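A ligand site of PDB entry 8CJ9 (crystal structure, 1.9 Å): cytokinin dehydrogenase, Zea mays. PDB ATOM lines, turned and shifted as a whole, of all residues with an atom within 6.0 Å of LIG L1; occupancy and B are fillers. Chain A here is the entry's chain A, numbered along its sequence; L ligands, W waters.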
ATOM      1  N   TRP A 105     -17.772   9.917  22.960  1.00  0.00           N
ATOM      2  CA  TRP A 105     -17.678   9.955  21.515  1.00  0.00           C
ATOM      3  C   TRP A 105     -17.323   8.599  20.913  1.00  0.00           C
ATOM      4  O   TRP A 105     -17.232   8.502  19.698  1.00  0.00           O
ATOM      5  CB  TRP A 105     -16.714  11.096  21.042  1.00  0.00           C
ATOM      6  CG  TRP A 105     -15.418  11.153  21.762  1.00  0.00           C
ATOM      7  CD1 TRP A 105     -14.255  10.535  21.419  1.00  0.00           C
ATOM      8  CD2 TRP A 105     -15.162  11.805  23.012  1.00  0.00           C
ATOM      9  NE1 TRP A 105     -13.291  10.753  22.374  1.00  0.00           N
ATOM     10  CE2 TRP A 105     -13.825  11.520  23.373  1.00  0.00           C
ATOM     11  CE3 TRP A 105     -15.935  12.623  23.855  1.00  0.00           C
ATOM     12  CZ2 TRP A 105     -13.235  12.034  24.537  1.00  0.00           C
ATOM     13  CZ3 TRP A 105     -15.364  13.092  25.032  1.00  0.00           C
ATOM     14  CH2 TRP A 105     -14.034  12.778  25.370  1.00  0.00           C
ATOM     15  N   ASP A 167     -13.939  21.686  32.154  1.00  0.00           N
ATOM     16  CA  ASP A 167     -14.071  22.918  31.364  1.00  0.00           C
ATOM     17  C   ASP A 167     -15.509  23.126  30.942  1.00  0.00           C
ATOM     18  O   ASP A 167     -15.870  24.242  30.638  1.00  0.00           O
ATOM     19  CB  ASP A 167     -13.217  22.848  30.090  1.00  0.00           C
ATOM     20  CG  ASP A 167     -11.745  22.717  30.322  1.00  0.00           C
ATOM     21  OD1 ASP A 167     -11.276  23.123  31.405  1.00  0.00           O
ATOM     22  OD2 ASP A 167     -11.060  22.209  29.427  1.00  0.00           O
ATOM     23  N   TYR A 168     -16.299  22.053  30.855  1.00  0.00           N
ATOM     24  CA  TYR A 168     -17.684  22.073  30.399  1.00  0.00           C
ATOM     25  C   TYR A 168     -18.580  21.619  31.537  1.00  0.00           C
ATOM     26  O   TYR A 168     -18.463  20.492  32.012  1.00  0.00           O
ATOM     27  CB  TYR A 168     -17.802  21.164  29.162  1.00  0.00           C
ATOM     28  CG  TYR A 168     -19.117  21.255  28.429  1.00  0.00           C
ATOM     29  CD1 TYR A 168     -19.418  22.348  27.623  1.00  0.00           C
ATOM     30  CD2 TYR A 168     -20.077  20.245  28.548  1.00  0.00           C
ATOM     31  CE1 TYR A 168     -20.640  22.437  26.961  1.00  0.00           C
ATOM     32  CE2 TYR A 168     -21.285  20.317  27.867  1.00  0.00           C
ATOM     33  CZ  TYR A 168     -21.564  21.425  27.076  1.00  0.00           C
ATOM     34  OH  TYR A 168     -22.752  21.525  26.406  1.00  0.00           O
ATOM     35  N   ILE A 182     -10.953  16.059  35.070  1.00  0.00           N
ATOM     36  CA  ILE A 182      -9.788  16.933  35.122  1.00  0.00           C
ATOM     37  C   ILE A 182     -10.145  18.345  34.620  1.00  0.00           C
ATOM     38  O   ILE A 182     -11.056  18.524  33.821  1.00  0.00           O
ATOM     39  CB  ILE A 182      -8.505  16.351  34.462  1.00  0.00           C
ATOM     40  CG1 ILE A 182      -8.610  16.290  32.913  1.00  0.00           C
ATOM     41  CG2 ILE A 182      -8.145  14.983  35.067  1.00  0.00           C
ATOM     42  CD1 ILE A 182      -7.223  15.940  32.142  1.00  0.00           C
ATOM     43  N   GLY A 183      -9.414  19.317  35.145  1.00  0.00           N
ATOM     44  CA  GLY A 183      -9.545  20.731  34.851  1.00  0.00           C
ATOM     45  C   GLY A 183      -8.370  21.484  35.429  1.00  0.00           C
ATOM     46  O   GLY A 183      -7.443  20.879  35.977  1.00  0.00           O
ATOM     47  N   ARG A 251      -4.363  35.034  29.639  1.00  0.00           N
ATOM     48  CA  ARG A 251      -3.793  34.196  28.580  1.00  0.00           C
ATOM     49  C   ARG A 251      -2.449  34.800  28.174  1.00  0.00           C
ATOM     50  O   ARG A 251      -2.362  35.984  27.916  1.00  0.00           O
ATOM     51  CB  ARG A 251      -4.746  34.016  27.385  1.00  0.00           C
ATOM     52  CG  ARG A 251      -5.853  33.012  27.668  1.00  0.00           C
ATOM     53  CD  ARG A 251      -6.590  32.632  26.409  1.00  0.00           C
ATOM     54  NE  ARG A 251      -7.742  31.791  26.700  1.00  0.00           N
ATOM     55  CZ  ARG A 251      -8.628  31.405  25.785  1.00  0.00           C
ATOM     56  NH1 ARG A 251      -9.670  30.672  26.139  1.00  0.00           N
ATOM     57  NH2 ARG A 251      -8.482  31.770  24.513  1.00  0.00           N
ATOM     58  N   GLU A 281      -4.149  26.163  32.918  1.00  0.00           N
ATOM     59  CA  GLU A 281      -4.358  25.388  31.702  1.00  0.00           C
ATOM     60  C   GLU A 281      -3.416  25.928  30.609  1.00  0.00           C
ATOM     61  O   GLU A 281      -2.562  26.784  30.864  1.00  0.00           O
ATOM     62  CB  GLU A 281      -5.833  25.350  31.261  1.00  0.00           C
ATOM     63  CG  GLU A 281      -6.627  24.290  32.024  1.00  0.00           C
ATOM     64  CD  GLU A 281      -8.022  23.925  31.537  1.00  0.00           C
ATOM     65  OE1 GLU A 281      -8.813  23.435  32.379  1.00  0.00           O
ATOM     66  OE2 GLU A 281      -8.347  24.142  30.346  1.00  0.00           O
ATOM     67  N   GLN A 283      -3.093  25.946  25.929  1.00  0.00           N
ATOM     68  CA  GLN A 283      -3.583  25.655  24.583  1.00  0.00           C
ATOM     69  C   GLN A 283      -2.461  25.721  23.591  1.00  0.00           C
ATOM     70  O   GLN A 283      -1.528  26.511  23.737  1.00  0.00           O
ATOM     71  CB  GLN A 283      -4.717  26.618  24.173  1.00  0.00           C
ATOM     72  CG  GLN A 283      -6.031  26.334  24.871  1.00  0.00           C
ATOM     73  CD  GLN A 283      -7.222  27.195  24.453  1.00  0.00           C
ATOM     74  OE1 GLN A 283      -8.117  27.468  25.269  1.00  0.00           O
ATOM     75  NE2 GLN A 283      -7.280  27.619  23.195  1.00  0.00           N
ATOM     76  N   ARG A 368     -17.466  29.692  31.269  1.00  0.00           N
ATOM     77  CA  ARG A 368     -16.882  30.323  30.079  1.00  0.00           C
ATOM     78  C   ARG A 368     -17.132  29.556  28.764  1.00  0.00           C
ATOM     79  O   ARG A 368     -17.335  30.183  27.726  1.00  0.00           O
ATOM     80  CB  ARG A 368     -15.371  30.598  30.281  1.00  0.00           C
ATOM     81  CG  ARG A 368     -14.486  29.330  30.289  1.00  0.00           C
ATOM     82  CD  ARG A 368     -13.125  29.494  30.933  1.00  0.00           C
ATOM     83  NE  ARG A 368     -12.457  28.194  30.959  1.00  0.00           N
ATOM     84  CZ  ARG A 368     -12.646  27.278  31.904  1.00  0.00           C
ATOM     85  NH1 ARG A 368     -13.433  27.540  32.946  1.00  0.00           N
ATOM     86  NH2 ARG A 368     -12.067  26.090  31.811  1.00  0.00           N
ATOM     87  N   VAL A 369     -17.152  28.212  28.802  1.00  0.00           N
ATOM     88  CA  VAL A 369     -17.343  27.393  27.605  1.00  0.00           C
ATOM     89  C   VAL A 369     -18.806  27.491  27.068  1.00  0.00           C
ATOM     90  O   VAL A 369     -19.000  27.282  25.868  1.00  0.00           O
ATOM     91  CB  VAL A 369     -16.837  25.938  27.805  1.00  0.00           C
ATOM     92  CG1 VAL A 369     -17.227  25.027  26.637  1.00  0.00           C
ATOM     93  CG2 VAL A 369     -15.323  25.916  27.964  1.00  0.00           C
ATOM     94  N   GLU A 372     -18.637  29.771  24.237  1.00  0.00           N
ATOM     95  CA  GLU A 372     -17.969  29.105  23.101  1.00  0.00           C
ATOM     96  C   GLU A 372     -18.909  28.174  22.337  1.00  0.00           C
ATOM     97  O   GLU A 372     -18.936  28.205  21.107  1.00  0.00           O
ATOM     98  CB  GLU A 372     -16.703  28.353  23.545  1.00  0.00           C
ATOM     99  CG  GLU A 372     -15.635  29.317  24.035  1.00  0.00           C
ATOM    100  CD  GLU A 372     -14.338  28.660  24.451  1.00  0.00           C
ATOM    101  OE1 GLU A 372     -14.163  28.403  25.662  1.00  0.00           O
ATOM    102  OE2 GLU A 372     -13.488  28.407  23.564  1.00  0.00           O
ATOM    103  N   GLU A 373     -19.727  27.394  23.055  1.00  0.00           N
ATOM    104  CA  GLU A 373     -20.718  26.502  22.485  1.00  0.00           C
ATOM    105  C   GLU A 373     -21.763  27.349  21.697  1.00  0.00           C
ATOM    106  O   GLU A 373     -22.113  27.006  20.562  1.00  0.00           O
ATOM    107  CB  GLU A 373     -21.405  25.682  23.579  1.00  0.00           C
ATOM    108  CG  GLU A 373     -22.521  24.804  23.054  1.00  0.00           C
ATOM    109  CD  GLU A 373     -23.349  24.058  24.077  1.00  0.00           C
ATOM    110  OE1 GLU A 373     -22.931  23.975  25.254  1.00  0.00           O
ATOM    111  OE2 GLU A 373     -24.408  23.532  23.697  1.00  0.00           O
ATOM    112  N   LEU A 376     -20.199  28.358  18.462  1.00  0.00           N
ATOM    113  CA  LEU A 376     -20.105  27.159  17.630  1.00  0.00           C
ATOM    114  C   LEU A 376     -21.484  26.726  17.054  1.00  0.00           C
ATOM    115  O   LEU A 376     -21.571  26.444  15.857  1.00  0.00           O
ATOM    116  CB  LEU A 376     -19.415  25.992  18.389  1.00  0.00           C
ATOM    117  CG  LEU A 376     -17.903  26.200  18.658  1.00  0.00           C
ATOM    118  CD1 LEU A 376     -17.358  25.131  19.590  1.00  0.00           C
ATOM    119  CD2 LEU A 376     -17.087  26.285  17.351  1.00  0.00           C
ATOM    120  N   TRP A 382     -21.095  22.908  16.038  1.00  0.00           N
ATOM    121  CA  TRP A 382     -21.176  22.197  17.323  1.00  0.00           C
ATOM    122  C   TRP A 382     -21.673  20.751  17.120  1.00  0.00           C
ATOM    123  O   TRP A 382     -20.981  19.817  17.521  1.00  0.00           O
ATOM    124  CB  TRP A 382     -22.074  22.962  18.310  1.00  0.00           C
ATOM    125  CG  TRP A 382     -22.154  22.326  19.670  1.00  0.00           C
ATOM    126  CD1 TRP A 382     -23.125  21.491  20.132  1.00  0.00           C
ATOM    127  CD2 TRP A 382     -21.188  22.449  20.721  1.00  0.00           C
ATOM    128  NE1 TRP A 382     -22.818  21.075  21.405  1.00  0.00           N
ATOM    129  CE2 TRP A 382     -21.641  21.649  21.798  1.00  0.00           C
ATOM    130  CE3 TRP A 382     -19.989  23.166  20.868  1.00  0.00           C
ATOM    131  CZ2 TRP A 382     -20.955  21.567  23.011  1.00  0.00           C
ATOM    132  CZ3 TRP A 382     -19.313  23.087  22.071  1.00  0.00           C
ATOM    133  CH2 TRP A 382     -19.793  22.300  23.129  1.00  0.00           C
ATOM    134  N   TRP A 388     -12.277  12.814  19.116  1.00  0.00           N
ATOM    135  CA  TRP A 388     -11.388  13.314  20.149  1.00  0.00           C
ATOM    136  C   TRP A 388     -10.398  12.291  20.717  1.00  0.00           C
ATOM    137  O   TRP A 388     -10.709  11.093  20.843  1.00  0.00           O
ATOM    138  CB  TRP A 388     -12.197  13.952  21.279  1.00  0.00           C
ATOM    139  CG  TRP A 388     -12.859  15.247  20.921  1.00  0.00           C
ATOM    140  CD1 TRP A 388     -12.859  15.879  19.719  1.00  0.00           C
ATOM    141  CD2 TRP A 388     -13.637  16.059  21.808  1.00  0.00           C
ATOM    142  NE1 TRP A 388     -13.563  17.061  19.799  1.00  0.00           N
ATOM    143  CE2 TRP A 388     -14.055  17.197  21.081  1.00  0.00           C
ATOM    144  CE3 TRP A 388     -14.011  15.946  23.165  1.00  0.00           C
ATOM    145  CZ2 TRP A 388     -14.827  18.215  21.657  1.00  0.00           C
ATOM    146  CZ3 TRP A 388     -14.747  16.963  23.736  1.00  0.00           C
ATOM    147  CH2 TRP A 388     -15.128  18.084  22.997  1.00  0.00           C
ATOM    148  N   ASN A 390      -7.358  12.093  23.957  1.00  0.00           N
ATOM    149  CA  ASN A 390      -6.833  12.675  25.186  1.00  0.00           C
ATOM    150  C   ASN A 390      -5.711  11.803  25.689  1.00  0.00           C
ATOM    151  O   ASN A 390      -5.877  10.588  25.841  1.00  0.00           O
ATOM    152  CB  ASN A 390      -7.942  12.824  26.238  1.00  0.00           C
ATOM    153  CG  ASN A 390      -9.110  13.664  25.771  1.00  0.00           C
ATOM    154  OD1 ASN A 390      -9.130  14.872  25.958  1.00  0.00           O
ATOM    155  ND2 ASN A 390     -10.104  13.046  25.145  1.00  0.00           N
ATOM    156  N   ILE A 418      -9.844  22.643  19.163  1.00  0.00           N
ATOM    157  CA  ILE A 418      -8.788  23.150  20.036  1.00  0.00           C
ATOM    158  C   ILE A 418      -7.875  22.048  20.551  1.00  0.00           C
ATOM    159  O   ILE A 418      -8.263  20.879  20.639  1.00  0.00           O
ATOM    160  CB  ILE A 418      -9.293  24.035  21.220  1.00  0.00           C
ATOM    161  CG1 ILE A 418     -10.297  23.293  22.110  1.00  0.00           C
ATOM    162  CG2 ILE A 418      -9.832  25.395  20.746  1.00  0.00           C
ATOM    163  CD1 ILE A 418     -10.214  23.684  23.541  1.00  0.00           C
ATOM    164  N   LEU A 420      -5.592  21.218  23.873  1.00  0.00           N
ATOM    165  CA  LEU A 420      -5.204  21.574  25.238  1.00  0.00           C
ATOM    166  C   LEU A 420      -3.881  20.933  25.605  1.00  0.00           C
ATOM    167  O   LEU A 420      -3.564  19.843  25.110  1.00  0.00           O
ATOM    168  CB  LEU A 420      -6.275  21.197  26.278  1.00  0.00           C
ATOM    169  CG  LEU A 420      -7.658  21.849  26.156  1.00  0.00           C
ATOM    170  CD1 LEU A 420      -8.578  21.306  27.246  1.00  0.00           C
ATOM    171  CD2 LEU A 420      -7.587  23.360  26.267  1.00  0.00           C
ATOM    172  N   TYR A 422      -1.511  21.055  29.369  1.00  0.00           N
ATOM    173  CA  TYR A 422      -1.197  21.565  30.697  1.00  0.00           C
ATOM    174  C   TYR A 422      -0.712  20.443  31.609  1.00  0.00           C
ATOM    175  O   TYR A 422      -1.174  19.315  31.480  1.00  0.00           O
ATOM    176  CB  TYR A 422      -2.379  22.345  31.326  1.00  0.00           C
ATOM    177  CG  TYR A 422      -3.666  21.570  31.537  1.00  0.00           C
ATOM    178  CD1 TYR A 422      -4.657  21.538  30.550  1.00  0.00           C
ATOM    179  CD2 TYR A 422      -3.931  20.923  32.738  1.00  0.00           C
ATOM    180  CE1 TYR A 422      -5.874  20.881  30.764  1.00  0.00           C
ATOM    181  CE2 TYR A 422      -5.129  20.240  32.956  1.00  0.00           C
ATOM    182  CZ  TYR A 422      -6.104  20.232  31.961  1.00  0.00           C
ATOM    183  OH  TYR A 422      -7.291  19.548  32.198  1.00  0.00           O
ATOM    184  N   ALA A 449      -1.419  16.738  30.375  1.00  0.00           N
ATOM    185  CA  ALA A 449      -2.653  16.336  29.740  1.00  0.00           C
ATOM    186  C   ALA A 449      -2.605  17.048  28.387  1.00  0.00           C
ATOM    187  O   ALA A 449      -2.328  18.253  28.325  1.00  0.00           O
ATOM    188  CB  ALA A 449      -3.848  16.806  30.549  1.00  0.00           C
ATOM    189  N   SER A 451      -4.948  17.261  24.953  1.00  0.00           N
ATOM    190  CA  SER A 451      -6.253  16.953  24.409  1.00  0.00           C
ATOM    191  C   SER A 451      -6.422  17.456  23.002  1.00  0.00           C
ATOM    192  O   SER A 451      -6.292  18.651  22.756  1.00  0.00           O
ATOM    193  CB  SER A 451      -7.364  17.462  25.322  1.00  0.00           C
ATOM    194  OG  SER A 451      -7.301  16.817  26.581  1.00  0.00           O
ATOM    195  N   LEU A 453      -8.994  18.089  20.702  1.00  0.00           N
ATOM    196  CA  LEU A 453     -10.427  18.302  20.641  1.00  0.00           C
ATOM    197  C   LEU A 453     -10.834  18.779  19.263  1.00  0.00           C
ATOM    198  O   LEU A 453     -11.320  19.880  19.105  1.00  0.00           O
ATOM    199  CB  LEU A 453     -10.914  19.212  21.786  1.00  0.00           C
ATOM    200  CG  LEU A 453     -10.343  18.885  23.198  1.00  0.00           C
ATOM    201  CD1 LEU A 453     -10.689  19.956  24.211  1.00  0.00           C
ATOM    202  CD2 LEU A 453     -10.802  17.490  23.705  1.00  0.00           C
ATOM    203  N   TYR A 486      -6.406   9.201  28.463  1.00  0.00           N
ATOM    204  CA  TYR A 486      -7.401   9.704  29.414  1.00  0.00           C
ATOM    205  C   TYR A 486      -8.696   9.609  28.620  1.00  0.00           C
ATOM    206  O   TYR A 486      -8.643   9.739  27.397  1.00  0.00           O
ATOM    207  CB  TYR A 486      -7.109  11.144  29.885  1.00  0.00           C
ATOM    208  CG  TYR A 486      -8.215  11.678  30.771  1.00  0.00           C
ATOM    209  CD1 TYR A 486      -8.615  10.992  31.917  1.00  0.00           C
ATOM    210  CD2 TYR A 486      -8.893  12.844  30.446  1.00  0.00           C
ATOM    211  CE1 TYR A 486      -9.680  11.438  32.704  1.00  0.00           C
ATOM    212  CE2 TYR A 486      -9.933  13.327  31.242  1.00  0.00           C
ATOM    213  CZ  TYR A 486     -10.327  12.615  32.362  1.00  0.00           C
ATOM    214  OH  TYR A 486     -11.352  13.083  33.149  1.00  0.00           O
ATOM    215  N   LEU A 487      -9.840   9.252  29.270  1.00  0.00           N
ATOM    216  CA  LEU A 487     -11.119   8.974  28.570  1.00  0.00           C
ATOM    217  C   LEU A 487     -10.826   7.858  27.502  1.00  0.00           C
ATOM    218  O   LEU A 487     -11.116   8.039  26.315  1.00  0.00           O
ATOM    219  CB  LEU A 487     -11.702  10.266  27.953  1.00  0.00           C
ATOM    220  CG  LEU A 487     -11.934  11.413  28.942  1.00  0.00           C
ATOM    221  CD1 LEU A 487     -11.913  12.749  28.251  1.00  0.00           C
ATOM    222  CD2 LEU A 487     -13.266  11.245  29.686  1.00  0.00           C
HETATM  223  C1  LIG L   1     -10.826  18.891  28.518  1.00  0.00           C
HETATM  224  C2  LIG L   1     -10.452  17.579  28.754  1.00  0.00           C
HETATM  225 CL1  LIG L   1      -9.091  17.271  29.803  1.00  0.00          CL
HETATM  226  C3  LIG L   1     -11.057  16.523  28.129  1.00  0.00           C
HETATM  227  C4  LIG L   1     -12.091  16.802  27.259  1.00  0.00           C
HETATM  228 CL2  LIG L   1     -12.882  15.469  26.447  1.00  0.00          CL
HETATM  229  C5  LIG L   1     -12.491  18.111  26.997  1.00  0.00           C
HETATM  230  C6  LIG L   1     -11.893  19.160  27.697  1.00  0.00           C
HETATM  231  N1  LIG L   1     -12.224  20.552  27.488  1.00  0.00           N
HETATM  232  C7  LIG L   1     -13.127  21.013  26.452  1.00  0.00           C
HETATM  233  O1  LIG L   1     -13.686  20.246  25.730  1.00  0.00           O
HETATM  234  N2  LIG L   1     -13.322  22.431  26.374  1.00  0.00           N
HETATM  235  C8  LIG L   1     -14.061  23.202  25.396  1.00  0.00           C
HETATM  236  C9  LIG L   1     -15.090  22.651  24.634  1.00  0.00           C
HETATM  237  C10 LIG L   1     -15.693  23.406  23.631  1.00  0.00           C
HETATM  238  C11 LIG L   1     -15.213  24.682  23.337  1.00  0.00           C
HETATM  239  C12 LIG L   1     -14.152  25.225  24.066  1.00  0.00           C
HETATM  240  C13 LIG L   1     -13.543  24.480  25.076  1.00  0.00           C
HETATM  241  C14 LIG L   1     -12.386  25.112  25.894  1.00  0.00           C
HETATM  242  O2  LIG L   1     -11.794  24.528  26.743  1.00  0.00           O
HETATM  243  N3  LIG L   1     -11.905  26.442  25.576  1.00  0.00           N
HETATM  244  P1  LG2 L   2     -22.092   9.733  29.221  1.00  0.00           P
HETATM  245  O1  LG2 L   2     -21.495  10.258  27.973  1.00  0.00           O
HETATM  246  O2  LG2 L   2     -23.607   9.667  29.105  1.00  0.00           O
HETATM  247  O3  LG2 L   2     -21.492   8.337  29.716  1.00  0.00           O
HETATM  248  C1  LG2 L   2     -20.073   8.121  29.780  1.00  0.00           C
HETATM  249  C2  LG2 L   2     -19.788   6.730  30.307  1.00  0.00           C
HETATM  250  O4  LG2 L   2     -20.030   6.687  31.732  1.00  0.00           O
HETATM  251  C3  LG2 L   2     -20.616   5.598  29.710  1.00  0.00           C
HETATM  252  O5  LG2 L   2     -19.895   4.373  29.690  1.00  0.00           O
HETATM  253  C4  LG2 L   2     -21.809   5.534  30.670  1.00  0.00           C
HETATM  254  O6  LG2 L   2     -22.538   4.305  30.623  1.00  0.00           O
HETATM  255  C5  LG2 L   2     -21.107   5.814  32.010  1.00  0.00           C
HETATM  256  N1  LG2 L   2     -21.936   6.452  33.029  1.00  0.00           N
HETATM  257  C6  LG2 L   2     -22.754   7.550  32.886  1.00  0.00           C
HETATM  258  N2  LG2 L   2     -23.322   7.936  34.003  1.00  0.00           N
HETATM  259  C7  LG2 L   2     -22.865   7.021  34.941  1.00  0.00           C
HETATM  260  C8  LG2 L   2     -23.127   6.860  36.314  1.00  0.00           C
HETATM  261  N3  LG2 L   2     -23.997   7.601  36.992  1.00  0.00           N
HETATM  262  N4  LG2 L   2     -22.502   5.841  36.963  1.00  0.00           N
HETATM  263  C9  LG2 L   2     -21.664   5.054  36.270  1.00  0.00           C
HETATM  264  N5  LG2 L   2     -21.343   5.110  34.976  1.00  0.00           N
HETATM  265  C10 LG2 L   2     -21.990   6.116  34.354  1.00  0.00           C
HETATM  266  N6  LG2 L   2     -13.708  15.573  30.856  1.00  0.00           N
HETATM  267  C11 LG2 L   2     -12.826  16.112  31.766  1.00  0.00           C
HETATM  268  O7  LG2 L   2     -12.347  15.455  32.690  1.00  0.00           O
HETATM  269  N7  LG2 L   2     -12.515  17.454  31.729  1.00  0.00           N
HETATM  270  C12 LG2 L   2     -13.078  18.396  30.872  1.00  0.00           C
HETATM  271  O8  LG2 L   2     -12.732  19.565  30.955  1.00  0.00           O
HETATM  272  C13 LG2 L   2     -14.055  17.824  29.931  1.00  0.00           C
HETATM  273  N8  LG2 L   2     -14.658  18.639  29.100  1.00  0.00           N
HETATM  274  C14 LG2 L   2     -15.581  18.095  28.208  1.00  0.00           C
HETATM  275  C15 LG2 L   2     -16.210  18.940  27.301  1.00  0.00           C
HETATM  276  C16 LG2 L   2     -17.174  18.476  26.405  1.00  0.00           C
HETATM  277  C17 LG2 L   2     -17.810  19.448  25.447  1.00  0.00           C
HETATM  278  C18 LG2 L   2     -17.540  17.106  26.435  1.00  0.00           C
HETATM  279  C19 LG2 L   2     -18.637  16.575  25.553  1.00  0.00           C
HETATM  280  C20 LG2 L   2     -16.891  16.256  27.331  1.00  0.00           C
HETATM  281  C21 LG2 L   2     -15.901  16.720  28.202  1.00  0.00           C
HETATM  282  N9  LG2 L   2     -15.201  15.873  29.100  1.00  0.00           N
HETATM  283  C22 LG2 L   2     -14.283  16.392  29.989  1.00  0.00           C
HETATM  284  C23 LG2 L   2     -15.423  14.412  29.122  1.00  0.00           C
HETATM  285  C24 LG2 L   2     -16.549  13.987  30.057  1.00  0.00           C
HETATM  286  O9  LG2 L   2     -16.240  14.368  31.406  1.00  0.00           O
HETATM  287  C25 LG2 L   2     -16.791  12.478  30.010  1.00  0.00           C
HETATM  288  O10 LG2 L   2     -17.047  12.121  28.658  1.00  0.00           O
HETATM  289  C26 LG2 L   2     -17.840  11.902  30.960  1.00  0.00           C
HETATM  290  O11 LG2 L   2     -18.246  10.596  30.534  1.00  0.00           O
HETATM  291  C27 LG2 L   2     -19.044  12.774  31.217  1.00  0.00           C
HETATM  292  O12 LG2 L   2     -20.029  12.504  30.214  1.00  0.00           O
HETATM  293  P2  LG2 L   2     -21.635  12.275  30.586  1.00  0.00           P
HETATM  294  O13 LG2 L   2     -22.406  12.725  31.767  1.00  0.00           O
HETATM  295  O14 LG2 L   2     -22.338  12.949  29.398  1.00  0.00           O
HETATM  296  O15 LG2 L   2     -21.801  10.696  30.453  1.00  0.00           O
HETATM  297  O   HOH W   1      -9.580  20.483  31.105  1.00  0.00           O
HETATM  298  O   HOH W   2     -10.577  25.400  29.062  1.00  0.00           O
HETATM  299  O   HOH W   3     -10.908  28.717  24.252  1.00  0.00           O
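OD1 of Asp 167 lies within salt-bridge range of NH2 of Arg 368, at 3.1 Å. OE1 of Glu 281 sits close to OD1 of Asp 167. OD1 of Asn 390 is in hydrogen-bond range of OG of Ser 451 (2.7 Å). N of Leu 420 sits at hydrogen-bond distance from O of Ser 451, at 2.9 Å. O of Tyr 422 is in hydrogen-bond range of N of Ala 449 (2.8 Å). The backbone carbonyl oxygen (O) of Asn 390 lies within hydrogen-bond range of the backbone NH (N) of Tyr 486, 3.0 Å away. The backbone carbonyl oxygen (O) of Ile 418 sits at hydrogen-bond distance from the backbone NH (N) of Leu 453, at 2.9 Å. The indole nitrogen (NE1) of Trp 105 is in hydrogen-bond range of the backbone carbonyl oxygen (O) of Trp 388 (3.0 Å).
OH of Tyr 486 is in hydrogen-bond range of O7 of LG2 L2. O of Ile 182 is in hydrogen-bond range of N7 of LG2 L2 (2.8 Å). N of Ile 182 is in hydrogen-bond range of O7 of LG2 L2, at 2.8 Å. The side-chain carboxylate of Asp 167 lies within hydrogen-bond range of a nitrogen (N1) of LIG L1, 2.8 Å away. An oxygen (O8) of LG2 L2 lies within hydrogen-bond range of the backbone NH (N) of Asp 167, at 2.7 Å. The side-chain carboxylate (OE1) of Glu 372 sits at hydrogen-bond distance from a nitrogen (N3) of LIG L1 (3.0 Å).
A nitrogen (N1) of LIG L1 sits close to a nitrogen (N8) of LG2 L2, at 3.5 Å.
Water W3 lies within hydrogen-bond range of the side-chain carboxylate (OE2) of Glu 372 (2.7 Å), a nitrogen (N3) of LIG L1 (2.8 Å), the guanidinium group (NH1) of Arg 251 (3.0 Å) and the side-chain amide oxygen (OE1) of Gln 283 (3.2 Å).
Trp 105 touches LIG L1. Ile 182 touches LIG L1 (CD1 to CL1, 3.3 Å). OE1 of Gln 283 touches N3 of LIG L1 (3.9 Å). CG2 of Val 369 touches C14 of LIG L1, 3.7 Å away. CZ3 of Trp 382 touches C10 of LIG L1, 3.95 Å away. CE3 of Trp 388 touches CL2 of LIG L1, at 3.5 Å. Asn 390 touches LIG L1. Ile 418 touches LIG L1 (CD1 to C14, 3.5 Å). Leu 420 touches LIG L1. Tyr 422 touches LIG L1. Ser 451 touches LIG L1. Leu 453 touches LIG L1. CD1 of Leu 487 touches CL2 of LIG L1 (3.4 Å). Hydrophobic or aromatic side chains within 4 Å of LIG L1: Trp 105, Ile 182, Val 369, Trp 382, Trp 388, Ile 418, Leu 420, Leu 453 and Leu 487. 15 residues have an atom within 4 Å of LIG L1: Trp 105, Asp 167, Ile 182, Gln 283, Val 369, Glu 372, Trp 382, Trp 388, Asn 390, Ile 418, Leu 420, Tyr 422, Ser 451, Leu 453 and Leu 487.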
